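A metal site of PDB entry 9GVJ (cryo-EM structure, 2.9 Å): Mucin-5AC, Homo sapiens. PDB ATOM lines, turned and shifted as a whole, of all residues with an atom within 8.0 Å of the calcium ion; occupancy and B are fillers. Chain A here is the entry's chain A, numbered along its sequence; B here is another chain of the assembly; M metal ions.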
ATOM      1  N   THR A 417      -6.065 -11.104  20.380  1.00  0.00           N
ATOM      2  CA  THR A 417      -5.309 -12.115  19.661  1.00  0.00           C
ATOM      3  C   THR A 417      -5.888 -13.506  19.916  1.00  0.00           C
ATOM      4  O   THR A 417      -6.883 -13.683  20.620  1.00  0.00           O
ATOM      5  CB  THR A 417      -3.837 -12.059  20.055  1.00  0.00           C
ATOM      6  OG1 THR A 417      -3.664 -12.609  21.369  1.00  0.00           O
ATOM      7  CG2 THR A 417      -3.343 -10.623  20.057  1.00  0.00           C
ATOM      8  N   PHE A 418      -5.245 -14.513  19.310  1.00  0.00           N
ATOM      9  CA  PHE A 418      -5.693 -15.893  19.467  1.00  0.00           C
ATOM     10  C   PHE A 418      -5.525 -16.381  20.905  1.00  0.00           C
ATOM     11  O   PHE A 418      -6.306 -17.216  21.367  1.00  0.00           O
ATOM     12  CB  PHE A 418      -4.922 -16.816  18.516  1.00  0.00           C
ATOM     13  CG  PHE A 418      -5.352 -16.712  17.081  1.00  0.00           C
ATOM     14  CD1 PHE A 418      -6.639 -17.032  16.704  1.00  0.00           C
ATOM     15  CD2 PHE A 418      -4.456 -16.304  16.114  1.00  0.00           C
ATOM     16  CE1 PHE A 418      -7.036 -16.947  15.384  1.00  0.00           C
ATOM     17  CE2 PHE A 418      -4.840 -16.202  14.791  1.00  0.00           C
ATOM     18  CZ  PHE A 418      -6.130 -16.531  14.424  1.00  0.00           C
ATOM     19  N   ASP A 419      -4.522 -15.865  21.612  1.00  0.00           N
ATOM     20  CA  ASP A 419      -4.242 -16.284  22.986  1.00  0.00           C
ATOM     21  C   ASP A 419      -4.968 -15.432  24.020  1.00  0.00           C
ATOM     22  O   ASP A 419      -4.735 -15.603  25.220  1.00  0.00           O
ATOM     23  CB  ASP A 419      -2.733 -16.242  23.238  1.00  0.00           C
ATOM     24  CG  ASP A 419      -1.973 -17.284  22.429  1.00  0.00           C
ATOM     25  OD1 ASP A 419      -2.604 -18.262  21.985  1.00  0.00           O
ATOM     26  OD2 ASP A 419      -0.757 -17.112  22.222  1.00  0.00           O
ATOM     27  N   GLY A 420      -5.837 -14.522  23.579  1.00  0.00           N
ATOM     28  CA  GLY A 420      -6.618 -13.701  24.481  1.00  0.00           C
ATOM     29  C   GLY A 420      -6.030 -12.355  24.815  1.00  0.00           C
ATOM     30  O   GLY A 420      -6.681 -11.567  25.509  1.00  0.00           O
ATOM     31  N   LYS A 421      -4.816 -12.059  24.364  1.00  0.00           N
ATOM     32  CA  LYS A 421      -4.215 -10.760  24.625  1.00  0.00           C
ATOM     33  C   LYS A 421      -4.987  -9.669  23.901  1.00  0.00           C
ATOM     34  O   LYS A 421      -5.342  -9.806  22.725  1.00  0.00           O
ATOM     35  CB  LYS A 421      -2.747 -10.743  24.187  1.00  0.00           C
ATOM     36  CG  LYS A 421      -2.009  -9.465  24.558  1.00  0.00           C
ATOM     37  CD  LYS A 421      -0.534  -9.580  24.265  1.00  0.00           C
ATOM     38  CE  LYS A 421       0.299  -9.156  25.459  1.00  0.00           C
ATOM     39  NZ  LYS A 421      -0.411  -8.158  26.310  1.00  0.00           N
ATOM     40  N   GLY A 538       0.684 -22.635  17.612  1.00  0.00           N
ATOM     41  CA  GLY A 538       2.118 -22.445  17.660  1.00  0.00           C
ATOM     42  C   GLY A 538       2.791 -22.234  16.327  1.00  0.00           C
ATOM     43  O   GLY A 538       4.030 -22.152  16.284  1.00  0.00           O
ATOM     44  N   THR A 540       1.243 -20.030  13.510  1.00  0.00           N
ATOM     45  CA  THR A 540       0.969 -18.740  12.895  1.00  0.00           C
ATOM     46  C   THR A 540       1.731 -17.635  13.624  1.00  0.00           C
ATOM     47  O   THR A 540       2.294 -17.837  14.696  1.00  0.00           O
ATOM     48  CB  THR A 540      -0.522 -18.448  12.902  1.00  0.00           C
ATOM     49  OG1 THR A 540      -1.027 -18.558  14.238  1.00  0.00           O
ATOM     50  CG2 THR A 540      -1.259 -19.437  12.005  1.00  0.00           C
ATOM     51  N   CYS A 544      -2.152 -11.213  15.375  1.00  0.00           N
ATOM     52  CA  CYS A 544      -3.027 -12.044  16.189  1.00  0.00           C
ATOM     53  C   CYS A 544      -2.266 -13.040  17.054  1.00  0.00           C
ATOM     54  O   CYS A 544      -2.870 -13.969  17.604  1.00  0.00           O
ATOM     55  CB  CYS A 544      -4.025 -12.786  15.289  1.00  0.00           C
ATOM     56  SG  CYS A 544      -5.333 -11.738  14.610  1.00  0.00           S
ATOM     57  N   GLY A 545      -0.953 -12.885  17.172  1.00  0.00           N
ATOM     58  CA  GLY A 545      -0.164 -13.754  18.018  1.00  0.00           C
ATOM     59  C   GLY A 545       0.213 -15.055  17.329  1.00  0.00           C
ATOM     60  O   GLY A 545      -0.104 -15.305  16.173  1.00  0.00           O
ATOM     61  N   ASN A 546       0.918 -15.899  18.089  1.00  0.00           N
ATOM     62  CA  ASN A 546       1.420 -17.162  17.584  1.00  0.00           C
ATOM     63  C   ASN A 546       0.546 -18.360  17.960  1.00  0.00           C
ATOM     64  O   ASN A 546       0.909 -19.497  17.653  1.00  0.00           O
ATOM     65  CB  ASN A 546       2.858 -17.397  18.048  1.00  0.00           C
ATOM     66  CG  ASN A 546       3.012 -17.206  19.544  1.00  0.00           C
ATOM     67  OD1 ASN A 546       2.133 -16.657  20.199  1.00  0.00           O
ATOM     68  ND2 ASN A 546       4.132 -17.668  20.087  1.00  0.00           N
ATOM     69  N   PHE A 547      -0.588 -18.123  18.623  1.00  0.00           N
ATOM     70  CA  PHE A 547      -1.579 -19.162  18.895  1.00  0.00           C
ATOM     71  C   PHE A 547      -0.975 -20.329  19.692  1.00  0.00           C
ATOM     72  O   PHE A 547      -1.252 -21.495  19.416  1.00  0.00           O
ATOM     73  CB  PHE A 547      -2.209 -19.654  17.603  1.00  0.00           C
ATOM     74  CG  PHE A 547      -3.501 -20.404  17.794  1.00  0.00           C
ATOM     75  CD1 PHE A 547      -4.204 -20.314  18.984  1.00  0.00           C
ATOM     76  CD2 PHE A 547      -4.010 -21.206  16.781  1.00  0.00           C
ATOM     77  CE1 PHE A 547      -5.390 -21.008  19.154  1.00  0.00           C
ATOM     78  CE2 PHE A 547      -5.182 -21.898  16.946  1.00  0.00           C
ATOM     79  CZ  PHE A 547      -5.879 -21.800  18.135  1.00  0.00           C
ATOM     80  N   ASN A 548      -0.149 -20.010  20.688  1.00  0.00           N
ATOM     81  CA  ASN A 548       0.501 -21.031  21.504  1.00  0.00           C
ATOM     82  C   ASN A 548       0.071 -20.935  22.971  1.00  0.00           C
ATOM     83  O   ASN A 548       0.808 -21.364  23.865  1.00  0.00           O
ATOM     84  CB  ASN A 548       2.017 -20.933  21.376  1.00  0.00           C
ATOM     85  CG  ASN A 548       2.584 -19.703  22.047  1.00  0.00           C
ATOM     86  OD1 ASN A 548       1.894 -18.706  22.242  1.00  0.00           O
ATOM     87  ND2 ASN A 548       3.871 -19.767  22.399  1.00  0.00           N
ATOM     88  N   SER A 549      -1.125 -20.394  23.217  1.00  0.00           N
ATOM     89  CA  SER A 549      -1.757 -20.335  24.538  1.00  0.00           C
ATOM     90  C   SER A 549      -0.981 -19.485  25.537  1.00  0.00           C
ATOM     91  O   SER A 549      -1.298 -19.508  26.730  1.00  0.00           O
ATOM     92  CB  SER A 549      -1.978 -21.739  25.113  1.00  0.00           C
ATOM     93  OG  SER A 549      -2.912 -22.469  24.341  1.00  0.00           O
ATOM     94  N   ILE A 550       0.012 -18.731  25.089  1.00  0.00           N
ATOM     95  CA  ILE A 550       0.812 -17.869  25.963  1.00  0.00           C
ATOM     96  C   ILE A 550       0.607 -16.437  25.518  1.00  0.00           C
ATOM     97  O   ILE A 550       0.820 -16.104  24.347  1.00  0.00           O
ATOM     98  CB  ILE A 550       2.306 -18.258  25.925  1.00  0.00           C
ATOM     99  CG1 ILE A 550       2.513 -19.656  26.500  1.00  0.00           C
ATOM    100  CG2 ILE A 550       3.136 -17.236  26.687  1.00  0.00           C
ATOM    101  CD1 ILE A 550       3.927 -20.146  26.407  1.00  0.00           C
ATOM    102  N   GLN A 551       0.177 -15.586  26.449  1.00  0.00           N
ATOM    103  CA  GLN A 551      -0.025 -14.171  26.140  1.00  0.00           C
ATOM    104  C   GLN A 551       1.267 -13.366  26.199  1.00  0.00           C
ATOM    105  O   GLN A 551       1.332 -12.290  25.605  1.00  0.00           O
ATOM    106  CB  GLN A 551      -1.044 -13.566  27.095  1.00  0.00           C
ATOM    107  CG  GLN A 551      -2.388 -14.269  27.107  1.00  0.00           C
ATOM    108  CD  GLN A 551      -3.440 -13.494  27.876  1.00  0.00           C
ATOM    109  OE1 GLN A 551      -3.144 -12.471  28.505  1.00  0.00           O
ATOM    110  NE2 GLN A 551      -4.677 -13.972  27.829  1.00  0.00           N
ATOM    111  N   ALA A 552       2.284 -13.860  26.914  1.00  0.00           N
ATOM    112  CA  ALA A 552       3.505 -13.093  27.100  1.00  0.00           C
ATOM    113  C   ALA A 552       4.223 -12.863  25.774  1.00  0.00           C
ATOM    114  O   ALA A 552       4.736 -11.765  25.516  1.00  0.00           O
ATOM    115  CB  ALA A 552       4.429 -13.809  28.093  1.00  0.00           C
ATOM    116  N   ASP A 553       4.285 -13.880  24.914  1.00  0.00           N
ATOM    117  CA  ASP A 553       5.036 -13.801  23.670  1.00  0.00           C
ATOM    118  C   ASP A 553       4.177 -13.342  22.492  1.00  0.00           C
ATOM    119  O   ASP A 553       4.625 -13.434  21.349  1.00  0.00           O
ATOM    120  CB  ASP A 553       5.681 -15.152  23.351  1.00  0.00           C
ATOM    121  CG  ASP A 553       4.661 -16.258  23.106  1.00  0.00           C
ATOM    122  OD1 ASP A 553       3.458 -16.040  23.356  1.00  0.00           O
ATOM    123  OD2 ASP A 553       5.068 -17.341  22.640  1.00  0.00           O
ATOM    124  N   ASP A 554       2.964 -12.838  22.740  1.00  0.00           N
ATOM    125  CA  ASP A 554       2.131 -12.359  21.651  1.00  0.00           C
ATOM    126  C   ASP A 554       2.610 -11.032  21.095  1.00  0.00           C
ATOM    127  O   ASP A 554       2.189 -10.649  20.002  1.00  0.00           O
ATOM    128  CB  ASP A 554       0.679 -12.229  22.128  1.00  0.00           C
ATOM    129  CG  ASP A 554      -0.145 -13.457  21.814  1.00  0.00           C
ATOM    130  OD1 ASP A 554       0.444 -14.504  21.479  1.00  0.00           O
ATOM    131  OD2 ASP A 554      -1.393 -13.373  21.897  1.00  0.00           O
ATOM    132  N   PHE A 555       3.477 -10.324  21.815  1.00  0.00           N
ATOM    133  CA  PHE A 555       4.085  -9.095  21.333  1.00  0.00           C
ATOM    134  C   PHE A 555       5.491  -9.327  20.787  1.00  0.00           C
ATOM    135  O   PHE A 555       6.287  -8.383  20.724  1.00  0.00           O
ATOM    136  CB  PHE A 555       4.122  -8.035  22.439  1.00  0.00           C
ATOM    137  CG  PHE A 555       2.818  -7.300  22.601  1.00  0.00           C
ATOM    138  CD1 PHE A 555       1.725  -7.622  21.816  1.00  0.00           C
ATOM    139  CD2 PHE A 555       2.696  -6.300  23.545  1.00  0.00           C
ATOM    140  CE1 PHE A 555       0.531  -6.947  21.967  1.00  0.00           C
ATOM    141  CE2 PHE A 555       1.505  -5.626  23.705  1.00  0.00           C
ATOM    142  CZ  PHE A 555       0.425  -5.945  22.915  1.00  0.00           C
ATOM    143  N   ARG A 556       5.814 -10.559  20.412  1.00  0.00           N
ATOM    144  CA  ARG A 556       7.135 -10.878  19.867  1.00  0.00           C
ATOM    145  C   ARG A 556       7.170 -10.552  18.385  1.00  0.00           C
ATOM    146  O   ARG A 556       6.338 -11.057  17.608  1.00  0.00           O
ATOM    147  CB  ARG A 556       7.464 -12.352  20.104  1.00  0.00           C
ATOM    148  CG  ARG A 556       8.642 -12.851  19.285  1.00  0.00           C
ATOM    149  CD  ARG A 556       8.946 -14.310  19.564  1.00  0.00           C
ATOM    150  NE  ARG A 556       9.495 -14.520  20.905  1.00  0.00           N
ATOM    151  CZ  ARG A 556       9.086 -15.459  21.738  1.00  0.00           C
ATOM    152  NH1 ARG A 556       8.130 -16.311  21.409  1.00  0.00           N
ATOM    153  NH2 ARG A 556       9.659 -15.547  22.933  1.00  0.00           N
ATOM    154  N   ASP B1014       3.797 -20.326  32.444  1.00  0.00           N
ATOM    155  CA  ASP B1014       3.857 -19.403  31.306  1.00  0.00           C
ATOM    156  C   ASP B1014       2.488 -19.134  30.683  1.00  0.00           C
ATOM    157  O   ASP B1014       2.410 -18.368  29.718  1.00  0.00           O
ATOM    158  CB  ASP B1014       4.811 -19.895  30.204  1.00  0.00           C
ATOM    159  CG  ASP B1014       6.268 -19.717  30.583  1.00  0.00           C
ATOM    160  OD1 ASP B1014       6.539 -19.177  31.676  1.00  0.00           O
ATOM    161  OD2 ASP B1014       7.142 -20.120  29.793  1.00  0.00           O
HETATM  162 CA    CA M   1       1.464 -16.453  22.271  1.00  0.00          CA
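OG1 of Thr 417 lies close to N of Asp 419. N of Ser 549 is in hydrogen-bond range of OD1 of Asp 419, at 2.9 Å. NH1 of Arg 556 lies within salt-bridge range of OD2 of Asp 553, 3.5 Å away. The backbone carbonyl oxygen (O) of Asn 546 is in hydrogen-bond range of the backbone NH (N) of Gly 538, at 3.1 Å. The side-chain carboxylate (OD2) of Asp 554 lies within hydrogen-bond range of the side-chain hydroxyl (OG1) of Thr 417 (2.5 Å). The backbone carbonyl oxygen of Asp 419 sits at hydrogen-bond distance from the side-chain amide nitrogen of Gln 551 (3.1 Å).
The nearest printed residue that does not touch the calcium ion is Gln 551 (4.5 Å).
The calcium ion is bound by OD1 of Asn 546. The calcium ion is bound by O of Ile 550 (2.2 Å). OD1 of Asn 548 is bound to the calcium ion, 2.3 Å away. OD1 of Asp 553 is bound to the calcium ion, at 2.3 Å. OD2 of Asp 419 is bound to the calcium ion, at 2.3 Å. The calcium ion is bound by the side-chain carboxylate (OD1) of Asp 554.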
